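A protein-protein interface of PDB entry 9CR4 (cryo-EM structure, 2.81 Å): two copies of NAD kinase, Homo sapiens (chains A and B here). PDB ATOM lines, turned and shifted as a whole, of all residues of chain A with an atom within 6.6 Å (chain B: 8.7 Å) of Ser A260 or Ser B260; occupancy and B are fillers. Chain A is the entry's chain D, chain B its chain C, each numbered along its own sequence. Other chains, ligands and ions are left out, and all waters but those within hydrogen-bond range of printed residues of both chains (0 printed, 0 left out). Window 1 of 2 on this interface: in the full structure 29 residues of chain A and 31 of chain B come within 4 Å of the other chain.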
ATOM      1  N   SER A 250      38.484  -2.202  23.230  1.00  0.00           N
ATOM      2  CA  SER A 250      37.185  -2.701  22.800  1.00  0.00           C
ATOM      3  C   SER A 250      36.466  -1.735  21.873  1.00  0.00           C
ATOM      4  O   SER A 250      35.588  -2.165  21.120  1.00  0.00           O
ATOM      5  CB  SER A 250      36.302  -2.989  24.014  1.00  0.00           C
ATOM      6  OG  SER A 250      36.101  -1.819  24.784  1.00  0.00           O
ATOM      7  N   THR A 251      36.806  -0.449  21.922  1.00  0.00           N
ATOM      8  CA  THR A 251      36.290   0.540  20.989  1.00  0.00           C
ATOM      9  C   THR A 251      37.260   0.821  19.852  1.00  0.00           C
ATOM     10  O   THR A 251      36.950   1.628  18.971  1.00  0.00           O
ATOM     11  CB  THR A 251      35.968   1.840  21.730  1.00  0.00           C
ATOM     12  OG1 THR A 251      37.154   2.338  22.359  1.00  0.00           O
ATOM     13  CG2 THR A 251      34.911   1.590  22.793  1.00  0.00           C
ATOM     14  N   ALA A 254      39.484  -3.584  17.423  1.00  0.00           N
ATOM     15  CA  ALA A 254      38.778  -4.776  17.883  1.00  0.00           C
ATOM     16  C   ALA A 254      37.274  -4.634  17.691  1.00  0.00           C
ATOM     17  O   ALA A 254      36.578  -5.622  17.438  1.00  0.00           O
ATOM     18  CB  ALA A 254      39.106  -5.050  19.349  1.00  0.00           C
ATOM     19  N   ALA A 255      36.754  -3.410  17.812  1.00  0.00           N
ATOM     20  CA  ALA A 255      35.325  -3.189  17.618  1.00  0.00           C
ATOM     21  C   ALA A 255      34.908  -3.421  16.174  1.00  0.00           C
ATOM     22  O   ALA A 255      33.803  -3.911  15.919  1.00  0.00           O
ATOM     23  CB  ALA A 255      34.942  -1.775  18.051  1.00  0.00           C
ATOM     24  N   GLY A 258      33.731  -7.070  15.207  1.00  0.00           N
ATOM     25  CA  GLY A 258      32.570  -7.681  15.817  1.00  0.00           C
ATOM     26  C   GLY A 258      32.596  -7.795  17.323  1.00  0.00           C
ATOM     27  O   GLY A 258      31.685  -8.406  17.892  1.00  0.00           O
ATOM     28  N   ALA A 259      33.599  -7.230  17.989  1.00  0.00           N
ATOM     29  CA  ALA A 259      33.685  -7.337  19.435  1.00  0.00           C
ATOM     30  C   ALA A 259      32.680  -6.411  20.112  1.00  0.00           C
ATOM     31  O   ALA A 259      32.279  -5.378  19.572  1.00  0.00           O
ATOM     32  CB  ALA A 259      35.098  -7.012  19.917  1.00  0.00           C
ATOM     33  N   SER A 260      32.275  -6.800  21.317  1.00  0.00           N
ATOM     34  CA  SER A 260      31.408  -5.968  22.132  1.00  0.00           C
ATOM     35  C   SER A 260      32.217  -4.855  22.792  1.00  0.00           C
ATOM     36  O   SER A 260      33.447  -4.903  22.872  1.00  0.00           O
ATOM     37  CB  SER A 260      30.692  -6.809  23.185  1.00  0.00           C
ATOM     38  OG  SER A 260      29.858  -7.778  22.578  1.00  0.00           O
ATOM     39  N   MET A 261      31.508  -3.844  23.276  1.00  0.00           N
ATOM     40  CA  MET A 261      32.125  -2.649  23.837  1.00  0.00           C
ATOM     41  C   MET A 261      32.197  -2.797  25.351  1.00  0.00           C
ATOM     42  O   MET A 261      31.169  -2.771  26.035  1.00  0.00           O
ATOM     43  CB  MET A 261      31.343  -1.406  23.427  1.00  0.00           C
ATOM     44  CG  MET A 261      31.505  -1.059  21.956  1.00  0.00           C
ATOM     45  SD  MET A 261      30.251   0.079  21.353  1.00  0.00           S
ATOM     46  CE  MET A 261      28.768  -0.846  21.728  1.00  0.00           C
ATOM     47  N   ILE A 262      33.412  -2.950  25.870  1.00  0.00           N
ATOM     48  CA  ILE A 262      33.643  -3.209  27.285  1.00  0.00           C
ATOM     49  C   ILE A 262      34.052  -1.911  27.965  1.00  0.00           C
ATOM     50  O   ILE A 262      34.927  -1.190  27.470  1.00  0.00           O
ATOM     51  CB  ILE A 262      34.718  -4.291  27.483  1.00  0.00           C
ATOM     52  CG1 ILE A 262      34.268  -5.609  26.856  1.00  0.00           C
ATOM     53  CG2 ILE A 262      35.019  -4.479  28.959  1.00  0.00           C
ATOM     54  CD1 ILE A 262      35.073  -6.804  27.299  1.00  0.00           C
ATOM     55  N   MET A 270      40.059  -9.583  26.155  1.00  0.00           N
ATOM     56  CA  MET A 270      39.200  -9.979  25.048  1.00  0.00           C
ATOM     57  C   MET A 270      39.988 -10.731  23.984  1.00  0.00           C
ATOM     58  O   MET A 270      41.186 -10.508  23.796  1.00  0.00           O
ATOM     59  CB  MET A 270      38.536  -8.759  24.413  1.00  0.00           C
ATOM     60  CG  MET A 270      37.990  -7.766  25.408  1.00  0.00           C
ATOM     61  SD  MET A 270      37.332  -6.310  24.587  1.00  0.00           S
ATOM     62  CE  MET A 270      36.067  -7.049  23.560  1.00  0.00           C
ATOM     63  N   THR A 272      39.232 -11.537  19.907  1.00  0.00           N
ATOM     64  CA  THR A 272      38.338 -11.243  18.799  1.00  0.00           C
ATOM     65  C   THR A 272      39.011 -11.606  17.481  1.00  0.00           C
ATOM     66  O   THR A 272      40.114 -11.113  17.190  1.00  0.00           O
ATOM     67  CB  THR A 272      37.939  -9.766  18.798  1.00  0.00           C
ATOM     68  OG1 THR A 272      37.363  -9.425  20.064  1.00  0.00           O
ATOM     69  CG2 THR A 272      36.928  -9.491  17.702  1.00  0.00           C
ATOM     70  N   ARG A 282      32.359 -16.597  17.890  1.00  0.00           N
ATOM     71  CA  ARG A 282      32.026 -15.318  18.486  1.00  0.00           C
ATOM     72  C   ARG A 282      33.155 -14.845  19.392  1.00  0.00           C
ATOM     73  O   ARG A 282      33.847 -15.663  20.005  1.00  0.00           O
ATOM     74  CB  ARG A 282      30.727 -15.435  19.292  1.00  0.00           C
ATOM     75  CG  ARG A 282      29.966 -14.135  19.477  1.00  0.00           C
ATOM     76  CD  ARG A 282      28.469 -14.375  19.524  1.00  0.00           C
ATOM     77  NE  ARG A 282      27.948 -14.787  18.226  1.00  0.00           N
ATOM     78  CZ  ARG A 282      26.660 -14.918  17.944  1.00  0.00           C
ATOM     79  NH1 ARG A 282      25.727 -14.685  18.852  1.00  0.00           N
ATOM     80  NH2 ARG A 282      26.299 -15.294  16.721  1.00  0.00           N
ATOM     81  N   PRO A 283      33.384 -13.536  19.477  1.00  0.00           N
ATOM     82  CA  PRO A 283      34.426 -13.035  20.376  1.00  0.00           C
ATOM     83  C   PRO A 283      34.155 -13.446  21.814  1.00  0.00           C
ATOM     84  O   PRO A 283      33.012 -13.456  22.274  1.00  0.00           O
ATOM     85  CB  PRO A 283      34.343 -11.517  20.198  1.00  0.00           C
ATOM     86  CG  PRO A 283      33.825 -11.341  18.823  1.00  0.00           C
ATOM     87  CD  PRO A 283      32.869 -12.475  18.593  1.00  0.00           C
ATOM     88  N   ILE A 284      35.223 -13.792  22.521  1.00  0.00           N
ATOM     89  CA  ILE A 284      35.134 -14.185  23.918  1.00  0.00           C
ATOM     90  C   ILE A 284      35.981 -13.230  24.738  1.00  0.00           C
ATOM     91  O   ILE A 284      36.923 -12.612  24.233  1.00  0.00           O
ATOM     92  CB  ILE A 284      35.592 -15.639  24.151  1.00  0.00           C
ATOM     93  CG1 ILE A 284      37.062 -15.799  23.773  1.00  0.00           C
ATOM     94  CG2 ILE A 284      34.742 -16.599  23.344  1.00  0.00           C
ATOM     95  CD1 ILE A 284      37.645 -17.134  24.161  1.00  0.00           C
ATOM     96  N   VAL A 285      35.636 -13.106  26.016  1.00  0.00           N
ATOM     97  CA  VAL A 285      36.412 -12.314  26.958  1.00  0.00           C
ATOM     98  C   VAL A 285      36.721 -13.191  28.165  1.00  0.00           C
ATOM     99  O   VAL A 285      35.858 -13.931  28.649  1.00  0.00           O
ATOM    100  CB  VAL A 285      35.676 -11.015  27.355  1.00  0.00           C
ATOM    101  CG1 VAL A 285      34.439 -11.304  28.155  1.00  0.00           C
ATOM    102  CG2 VAL A 285      36.601 -10.082  28.093  1.00  0.00           C
ATOM    103  N   SER B 245      21.955  -9.183  31.665  1.00  0.00           N
ATOM    104  CA  SER B 245      22.270 -10.547  32.063  1.00  0.00           C
ATOM    105  C   SER B 245      23.632 -10.603  32.739  1.00  0.00           C
ATOM    106  O   SER B 245      24.444  -9.681  32.635  1.00  0.00           O
ATOM    107  CB  SER B 245      22.252 -11.487  30.857  1.00  0.00           C
ATOM    108  OG  SER B 245      23.194 -11.074  29.886  1.00  0.00           O
ATOM    109  N   THR B 246      23.867 -11.709  33.437  1.00  0.00           N
ATOM    110  CA  THR B 246      25.143 -11.994  34.074  1.00  0.00           C
ATOM    111  C   THR B 246      26.075 -12.690  33.089  1.00  0.00           C
ATOM    112  O   THR B 246      25.657 -13.101  32.005  1.00  0.00           O
ATOM    113  CB  THR B 246      24.920 -12.868  35.306  1.00  0.00           C
ATOM    114  OG1 THR B 246      24.431 -14.149  34.897  1.00  0.00           O
ATOM    115  CG2 THR B 246      23.917 -12.231  36.237  1.00  0.00           C
ATOM    116  N   PRO B 247      27.361 -12.827  33.433  1.00  0.00           N
ATOM    117  CA  PRO B 247      28.252 -13.628  32.581  1.00  0.00           C
ATOM    118  C   PRO B 247      27.793 -15.061  32.408  1.00  0.00           C
ATOM    119  O   PRO B 247      28.037 -15.658  31.352  1.00  0.00           O
ATOM    120  CB  PRO B 247      29.592 -13.553  33.320  1.00  0.00           C
ATOM    121  CG  PRO B 247      29.541 -12.265  34.027  1.00  0.00           C
ATOM    122  CD  PRO B 247      28.115 -12.082  34.455  1.00  0.00           C
ATOM    123  N   GLY B 249      24.824 -16.003  31.956  1.00  0.00           N
ATOM    124  CA  GLY B 249      23.826 -15.953  30.913  1.00  0.00           C
ATOM    125  C   GLY B 249      24.347 -15.558  29.555  1.00  0.00           C
ATOM    126  O   GLY B 249      23.559 -15.472  28.608  1.00  0.00           O
ATOM    127  N   SER B 250      25.652 -15.313  29.424  1.00  0.00           N
ATOM    128  CA  SER B 250      26.240 -14.989  28.131  1.00  0.00           C
ATOM    129  C   SER B 250      26.235 -16.171  27.175  1.00  0.00           C
ATOM    130  O   SER B 250      26.513 -15.987  25.986  1.00  0.00           O
ATOM    131  CB  SER B 250      27.670 -14.483  28.317  1.00  0.00           C
ATOM    132  OG  SER B 250      28.470 -15.449  28.975  1.00  0.00           O
ATOM    133  N   THR B 251      25.941 -17.372  27.667  1.00  0.00           N
ATOM    134  CA  THR B 251      25.783 -18.567  26.849  1.00  0.00           C
ATOM    135  C   THR B 251      24.322 -19.004  26.826  1.00  0.00           C
ATOM    136  O   THR B 251      24.002 -20.193  26.882  1.00  0.00           O
ATOM    137  CB  THR B 251      26.678 -19.692  27.357  1.00  0.00           C
ATOM    138  OG1 THR B 251      26.285 -20.053  28.687  1.00  0.00           O
ATOM    139  CG2 THR B 251      28.131 -19.242  27.371  1.00  0.00           C
ATOM    140  N   ALA B 252      23.425 -18.029  26.747  1.00  0.00           N
ATOM    141  CA  ALA B 252      21.988 -18.243  26.860  1.00  0.00           C
ATOM    142  C   ALA B 252      21.315 -17.332  25.839  1.00  0.00           C
ATOM    143  O   ALA B 252      21.940 -16.888  24.871  1.00  0.00           O
ATOM    144  CB  ALA B 252      21.510 -18.003  28.299  1.00  0.00           C
ATOM    145  N   ALA B 254      20.842 -14.447  25.787  1.00  0.00           N
ATOM    146  CA  ALA B 254      21.665 -13.273  25.521  1.00  0.00           C
ATOM    147  C   ALA B 254      22.601 -13.515  24.346  1.00  0.00           C
ATOM    148  O   ALA B 254      22.830 -12.616  23.529  1.00  0.00           O
ATOM    149  CB  ALA B 254      22.460 -12.893  26.770  1.00  0.00           C
ATOM    150  N   ALA B 255      23.153 -14.727  24.244  1.00  0.00           N
ATOM    151  CA  ALA B 255      24.045 -15.047  23.134  1.00  0.00           C
ATOM    152  C   ALA B 255      23.308 -15.068  21.804  1.00  0.00           C
ATOM    153  O   ALA B 255      23.888 -14.708  20.773  1.00  0.00           O
ATOM    154  CB  ALA B 255      24.729 -16.391  23.375  1.00  0.00           C
ATOM    155  N   ALA B 256      22.043 -15.486  21.801  1.00  0.00           N
ATOM    156  CA  ALA B 256      21.267 -15.509  20.569  1.00  0.00           C
ATOM    157  C   ALA B 256      21.023 -14.119  20.002  1.00  0.00           C
ATOM    158  O   ALA B 256      20.640 -14.006  18.833  1.00  0.00           O
ATOM    159  CB  ALA B 256      19.932 -16.213  20.804  1.00  0.00           C
ATOM    160  N   ALA B 257      21.234 -13.068  20.791  1.00  0.00           N
ATOM    161  CA  ALA B 257      21.049 -11.697  20.345  1.00  0.00           C
ATOM    162  C   ALA B 257      22.343 -11.057  19.861  1.00  0.00           C
ATOM    163  O   ALA B 257      22.356  -9.859  19.561  1.00  0.00           O
ATOM    164  CB  ALA B 257      20.436 -10.860  21.468  1.00  0.00           C
ATOM    165  N   GLY B 258      23.425 -11.824  19.773  1.00  0.00           N
ATOM    166  CA  GLY B 258      24.697 -11.311  19.313  1.00  0.00           C
ATOM    167  C   GLY B 258      25.684 -10.933  20.392  1.00  0.00           C
ATOM    168  O   GLY B 258      26.699 -10.300  20.080  1.00  0.00           O
ATOM    169  N   ALA B 259      25.426 -11.297  21.643  1.00  0.00           N
ATOM    170  CA  ALA B 259      26.317 -10.940  22.735  1.00  0.00           C
ATOM    171  C   ALA B 259      27.572 -11.800  22.721  1.00  0.00           C
ATOM    172  O   ALA B 259      27.531 -12.997  22.425  1.00  0.00           O
ATOM    173  CB  ALA B 259      25.607 -11.087  24.080  1.00  0.00           C
ATOM    174  N   SER B 260      28.699 -11.172  23.045  1.00  0.00           N
ATOM    175  CA  SER B 260      29.941 -11.906  23.207  1.00  0.00           C
ATOM    176  C   SER B 260      29.866 -12.797  24.442  1.00  0.00           C
ATOM    177  O   SER B 260      29.168 -12.501  25.415  1.00  0.00           O
ATOM    178  CB  SER B 260      31.123 -10.944  23.318  1.00  0.00           C
ATOM    179  OG  SER B 260      30.964 -10.067  24.420  1.00  0.00           O
ATOM    180  N   MET B 261      30.601 -13.902  24.396  1.00  0.00           N
ATOM    181  CA  MET B 261      30.528 -14.934  25.423  1.00  0.00           C
ATOM    182  C   MET B 261      31.558 -14.629  26.505  1.00  0.00           C
ATOM    183  O   MET B 261      32.765 -14.627  26.243  1.00  0.00           O
ATOM    184  CB  MET B 261      30.741 -16.313  24.806  1.00  0.00           C
ATOM    185  CG  MET B 261      29.707 -16.642  23.740  1.00  0.00           C
ATOM    186  SD  MET B 261      29.879 -18.284  23.028  1.00  0.00           S
ATOM    187  CE  MET B 261      31.591 -18.245  22.517  1.00  0.00           C
ATOM    188  N   ILE B 262      31.075 -14.374  27.715  1.00  0.00           N
ATOM    189  CA  ILE B 262      31.913 -13.939  28.823  1.00  0.00           C
ATOM    190  C   ILE B 262      32.171 -15.119  29.750  1.00  0.00           C
ATOM    191  O   ILE B 262      31.244 -15.857  30.104  1.00  0.00           O
ATOM    192  CB  ILE B 262      31.252 -12.779  29.586  1.00  0.00           C
ATOM    193  CG1 ILE B 262      31.033 -11.583  28.660  1.00  0.00           C
ATOM    194  CG2 ILE B 262      32.089 -12.382  30.789  1.00  0.00           C
ATOM    195  CD1 ILE B 262      30.648 -10.312  29.381  1.00  0.00           C
ATOM    196  N   HIS B 263      33.428 -15.301  30.137  1.00  0.00           N
ATOM    197  CA  HIS B 263      33.763 -16.327  31.112  1.00  0.00           C
ATOM    198  C   HIS B 263      33.164 -15.964  32.469  1.00  0.00           C
ATOM    199  O   HIS B 263      33.174 -14.791  32.857  1.00  0.00           O
ATOM    200  CB  HIS B 263      35.279 -16.480  31.223  1.00  0.00           C
ATOM    201  CG  HIS B 263      35.711 -17.643  32.059  1.00  0.00           C
ATOM    202  ND1 HIS B 263      35.799 -17.580  33.433  1.00  0.00           N
ATOM    203  CD2 HIS B 263      36.085 -18.897  31.716  1.00  0.00           C
ATOM    204  CE1 HIS B 263      36.206 -18.745  33.901  1.00  0.00           C
ATOM    205  NE2 HIS B 263      36.385 -19.563  32.880  1.00  0.00           N
ATOM    206  N   MET B 270      26.114  -7.381  31.630  1.00  0.00           N
ATOM    207  CA  MET B 270      25.924  -7.194  30.201  1.00  0.00           C
ATOM    208  C   MET B 270      24.583  -6.534  29.909  1.00  0.00           C
ATOM    209  O   MET B 270      23.613  -6.704  30.651  1.00  0.00           O
ATOM    210  CB  MET B 270      26.000  -8.529  29.464  1.00  0.00           C
ATOM    211  CG  MET B 270      27.155  -9.405  29.889  1.00  0.00           C
ATOM    212  SD  MET B 270      27.173 -10.960  28.988  1.00  0.00           S
ATOM    213  CE  MET B 270      27.296 -10.365  27.307  1.00  0.00           C
ATOM    214  N   ILE B 271      24.540  -5.774  28.818  1.00  0.00           N
ATOM    215  CA  ILE B 271      23.308  -5.190  28.297  1.00  0.00           C
ATOM    216  C   ILE B 271      23.264  -5.488  26.806  1.00  0.00           C
ATOM    217  O   ILE B 271      24.042  -4.917  26.032  1.00  0.00           O
ATOM    218  CB  ILE B 271      23.216  -3.681  28.558  1.00  0.00           C
ATOM    219  CG1 ILE B 271      23.172  -3.401  30.059  1.00  0.00           C
ATOM    220  CG2 ILE B 271      21.995  -3.099  27.883  1.00  0.00           C
ATOM    221  CD1 ILE B 271      23.074  -1.936  30.400  1.00  0.00           C
ATOM    222  N   THR B 272      22.361  -6.378  26.401  1.00  0.00           N
ATOM    223  CA  THR B 272      22.284  -6.848  25.022  1.00  0.00           C
ATOM    224  C   THR B 272      20.872  -6.624  24.497  1.00  0.00           C
ATOM    225  O   THR B 272      19.905  -7.148  25.085  1.00  0.00           O
ATOM    226  CB  THR B 272      22.666  -8.324  24.926  1.00  0.00           C
ATOM    227  OG1 THR B 272      23.968  -8.518  25.489  1.00  0.00           O
ATOM    228  CG2 THR B 272      22.682  -8.771  23.476  1.00  0.00           C
ATOM    229  N   PRO B 273      20.699  -5.872  23.417  1.00  0.00           N
ATOM    230  CA  PRO B 273      19.361  -5.646  22.864  1.00  0.00           C
ATOM    231  C   PRO B 273      18.877  -6.844  22.058  1.00  0.00           C
ATOM    232  O   PRO B 273      19.645  -7.727  21.675  1.00  0.00           O
ATOM    233  CB  PRO B 273      19.562  -4.429  21.963  1.00  0.00           C
ATOM    234  CG  PRO B 273      20.974  -4.546  21.523  1.00  0.00           C
ATOM    235  CD  PRO B 273      21.730  -5.118  22.686  1.00  0.00           C
ATOM    236  N   ARG B 282      25.296  -1.944  19.662  1.00  0.00           N
ATOM    237  CA  ARG B 282      25.909  -3.229  19.948  1.00  0.00           C
ATOM    238  C   ARG B 282      25.843  -3.507  21.439  1.00  0.00           C
ATOM    239  O   ARG B 282      25.717  -2.580  22.246  1.00  0.00           O
ATOM    240  CB  ARG B 282      27.370  -3.243  19.477  1.00  0.00           C
ATOM    241  CG  ARG B 282      27.571  -2.632  18.111  1.00  0.00           C
ATOM    242  CD  ARG B 282      29.035  -2.600  17.762  1.00  0.00           C
ATOM    243  NE  ARG B 282      29.608  -3.936  17.821  1.00  0.00           N
ATOM    244  CZ  ARG B 282      29.575  -4.801  16.818  1.00  0.00           C
ATOM    245  NH1 ARG B 282      29.030  -4.489  15.654  1.00  0.00           N
ATOM    246  NH2 ARG B 282      30.094  -6.013  16.989  1.00  0.00           N
ATOM    247  N   PRO B 283      25.906  -4.777  21.837  1.00  0.00           N
ATOM    248  CA  PRO B 283      25.872  -5.096  23.267  1.00  0.00           C
ATOM    249  C   PRO B 283      27.036  -4.458  24.003  1.00  0.00           C
ATOM    250  O   PRO B 283      28.156  -4.393  23.496  1.00  0.00           O
ATOM    251  CB  PRO B 283      25.960  -6.627  23.291  1.00  0.00           C
ATOM    252  CG  PRO B 283      26.497  -7.004  21.952  1.00  0.00           C
ATOM    253  CD  PRO B 283      25.946  -5.994  21.011  1.00  0.00           C
ATOM    254  N   ILE B 284      26.760  -3.982  25.211  1.00  0.00           N
ATOM    255  CA  ILE B 284      27.778  -3.386  26.061  1.00  0.00           C
ATOM    256  C   ILE B 284      27.839  -4.179  27.355  1.00  0.00           C
ATOM    257  O   ILE B 284      26.880  -4.859  27.735  1.00  0.00           O
ATOM    258  CB  ILE B 284      27.506  -1.897  26.355  1.00  0.00           C
ATOM    259  CG1 ILE B 284      26.248  -1.741  27.205  1.00  0.00           C
ATOM    260  CG2 ILE B 284      27.359  -1.117  25.065  1.00  0.00           C
ATOM    261  CD1 ILE B 284      26.000  -0.326  27.659  1.00  0.00           C
ATOM    262  N   VAL B 285      28.979  -4.097  28.029  1.00  0.00           N
ATOM    263  CA  VAL B 285      29.153  -4.710  29.337  1.00  0.00           C
ATOM    264  C   VAL B 285      29.719  -3.655  30.280  1.00  0.00           C
ATOM    265  O   VAL B 285      30.606  -2.880  29.906  1.00  0.00           O
ATOM    266  CB  VAL B 285      30.048  -5.966  29.269  1.00  0.00           C
ATOM    267  CG1 VAL B 285      31.461  -5.616  28.901  1.00  0.00           C
ATOM    268  CG2 VAL B 285      29.993  -6.731  30.566  1.00  0.00           C
ATOM    269  N   TRP B 343      34.701 -24.617  30.889  1.00  0.00           N
ATOM    270  CA  TRP B 343      33.895 -23.673  30.123  1.00  0.00           C
ATOM    271  C   TRP B 343      34.172 -23.778  28.630  1.00  0.00           C
ATOM    272  O   TRP B 343      33.241 -23.739  27.817  1.00  0.00           O
ATOM    273  CB  TRP B 343      34.144 -22.249  30.617  1.00  0.00           C
ATOM    274  CG  TRP B 343      33.292 -21.232  29.937  1.00  0.00           C
ATOM    275  CD1 TRP B 343      31.948 -21.072  30.072  1.00  0.00           C
ATOM    276  CD2 TRP B 343      33.729 -20.211  29.035  1.00  0.00           C
ATOM    277  NE1 TRP B 343      31.515 -20.028  29.296  1.00  0.00           N
ATOM    278  CE2 TRP B 343      32.591 -19.480  28.651  1.00  0.00           C
ATOM    279  CE3 TRP B 343      34.972 -19.850  28.510  1.00  0.00           C
ATOM    280  CZ2 TRP B 343      32.658 -18.410  27.767  1.00  0.00           C
ATOM    281  CZ3 TRP B 343      35.036 -18.786  27.634  1.00  0.00           C
ATOM    282  CH2 TRP B 343      33.886 -18.079  27.271  1.00  0.00           C
ATOM    283  N   LEU B 347      31.643 -24.850  25.503  1.00  0.00           N
ATOM    284  CA  LEU B 347      31.367 -24.047  24.316  1.00  0.00           C
ATOM    285  C   LEU B 347      31.367 -24.904  23.056  1.00  0.00           C
ATOM    286  O   LEU B 347      30.486 -24.770  22.199  1.00  0.00           O
ATOM    287  CB  LEU B 347      32.395 -22.924  24.195  1.00  0.00           C
ATOM    288  CG  LEU B 347      32.340 -21.788  25.213  1.00  0.00           C
ATOM    289  CD1 LEU B 347      33.558 -20.898  25.069  1.00  0.00           C
ATOM    290  CD2 LEU B 347      31.074 -20.984  25.025  1.00  0.00           C
ATOM    291  N   LEU B 351      27.476 -25.347  22.265  1.00  0.00           N
ATOM    292  CA  LEU B 351      27.176 -24.207  21.409  1.00  0.00           C
ATOM    293  C   LEU B 351      27.969 -24.203  20.108  1.00  0.00           C
ATOM    294  O   LEU B 351      27.734 -23.331  19.264  1.00  0.00           O
ATOM    295  CB  LEU B 351      27.430 -22.902  22.172  1.00  0.00           C
ATOM    296  CG  LEU B 351      26.562 -21.702  21.791  1.00  0.00           C
ATOM    297  CD1 LEU B 351      25.096 -22.099  21.724  1.00  0.00           C
ATOM    298  CD2 LEU B 351      26.765 -20.561  22.774  1.00  0.00           C
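The backbone carbonyl oxygen (O) of Ala B255 sits at hydrogen-bond distance from the guanidinium group (NH1) of Arg A282, 2.7 Å away.
OG of Ser B260 lies within hydrogen-bond range of OG of Ser A260, at 3.1 Å.
The backbone NH of Met B261 sits at hydrogen-bond distance from the backbone carbonyl oxygen of Pro A283 (3.2 Å).
The backbone carbonyl oxygen (O) of Met B261 is in hydrogen-bond range of the backbone NH (N) of Val A285.
N of His B263 sits at hydrogen-bond distance from O of Val A285 (3.2 Å).
The backbone carbonyl oxygen of Gly A258 lies within hydrogen-bond range of the guanidinium group of Arg B282, 3.0 Å away.
NH2 of Arg B282 is in hydrogen-bond range of O of Ala A259 (3.4 Å).
The backbone carbonyl oxygen (O) of Pro B283 sits at hydrogen-bond distance from the backbone NH (N) of Met A261 (3.4 Å).
The backbone NH of Val B285 is in hydrogen-bond range of the backbone carbonyl oxygen of Met A261, 3.2 Å away.
The side-chain hydroxyl (OG) of Ser B250 sits at hydrogen-bond distance from the backbone carbonyl oxygen (O) of Ile B262, 3.0 Å away.
The backbone NH (N) of Ala B259 sits close to the backbone carbonyl oxygen (O) of Ala B254 (3.5 Å).
The backbone NH of Ile B271 sits at hydrogen-bond distance from the backbone carbonyl oxygen of Ile B284.
The side-chain hydroxyl (OG) of Ser A250 is in hydrogen-bond range of the backbone carbonyl oxygen (O) of Ile A262, 3.0 Å away.
N of Ala A259 lies close to O of Ala A254, at 3.4 Å.
Among the printed residues, pairs that only touch across the chains: Pro A283 with Ser B260 (3.3 Å), Arg A282 with Ala B259 (3.3 Å), Ile A284 with Met B261 (3.3 Å), Met A261 with Ile B284 (3.4 Å), Val A285 with Ile B262 (3.5 Å), Ile A262 with Val B285 (3.5 Å), Ser A260 with Pro B283 (3.5 Å), Met A261 with Arg B282 (3.5 Å) and Arg A282 with Gly B258 (3.6 Å).
Ala A255 touches none of the printed residues of chain B.
Printed residues of chain B within 4 Å of Gly A258: Arg B282.
Ala A259 touches just one residue of chain B: Arg B282.
Ser A260 touches just these residues of chain B: Ser B260 (3.1 Å) and Pro B283 (3.5 Å).
Of chain A, only Ser A260 and Pro A283 come within 4 Å of Ser B260.
Of the printed residues of chain A, Ile B262 touches Val A285.
The nearest residue of chain A that does not touch Ser B260 is Arg A282 (4.3 Å).
The nearest printed residue of chain B that does not touch Arg A282 is Met B261 (4.3 Å).
Of the 15 printed residues of chain A, 9 touch a printed residue of chain B.
Hydrophobic or aromatic side chains of chain A that line the printed part of chain B: Met A261, Ile A262, Ile A284 and Val A285.
Hydrophobic or aromatic side chains of chain B within 4 Å of the printed part of chain A: Met B261, Ile B262, His B263, Pro B283, Ile B284 and Val B285.
Among the printed residues, 18 pairs touch across the chains.
Among the printed residues, no Asp or Glu carboxylate lies within 4 Å of a Lys or Arg side-chain nitrogen of the other chain.
Ala A259 touches Arg B282, and with the chains exchanged Arg A282 touches Ala B259.
Met A261 touches Pro B283, and with the chains exchanged Pro A283 touches Met B261.
Met A261 touches Ile B284, and with the chains exchanged Ile A284 touches Met B261.
Arg A282 touches Ala B255, but with the chains exchanged Ala A255 does not touch Arg B282 (4.4 Å).
Positions printed for both chains: 250, 251, 254, 255, 258, 259, 260, 261, 262, 270, 272, 282, 283, 284 and 285.
Of the 18 pairs that touch across the chains among the printed residues, 15 have their exchanged pair printed and touching as well.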
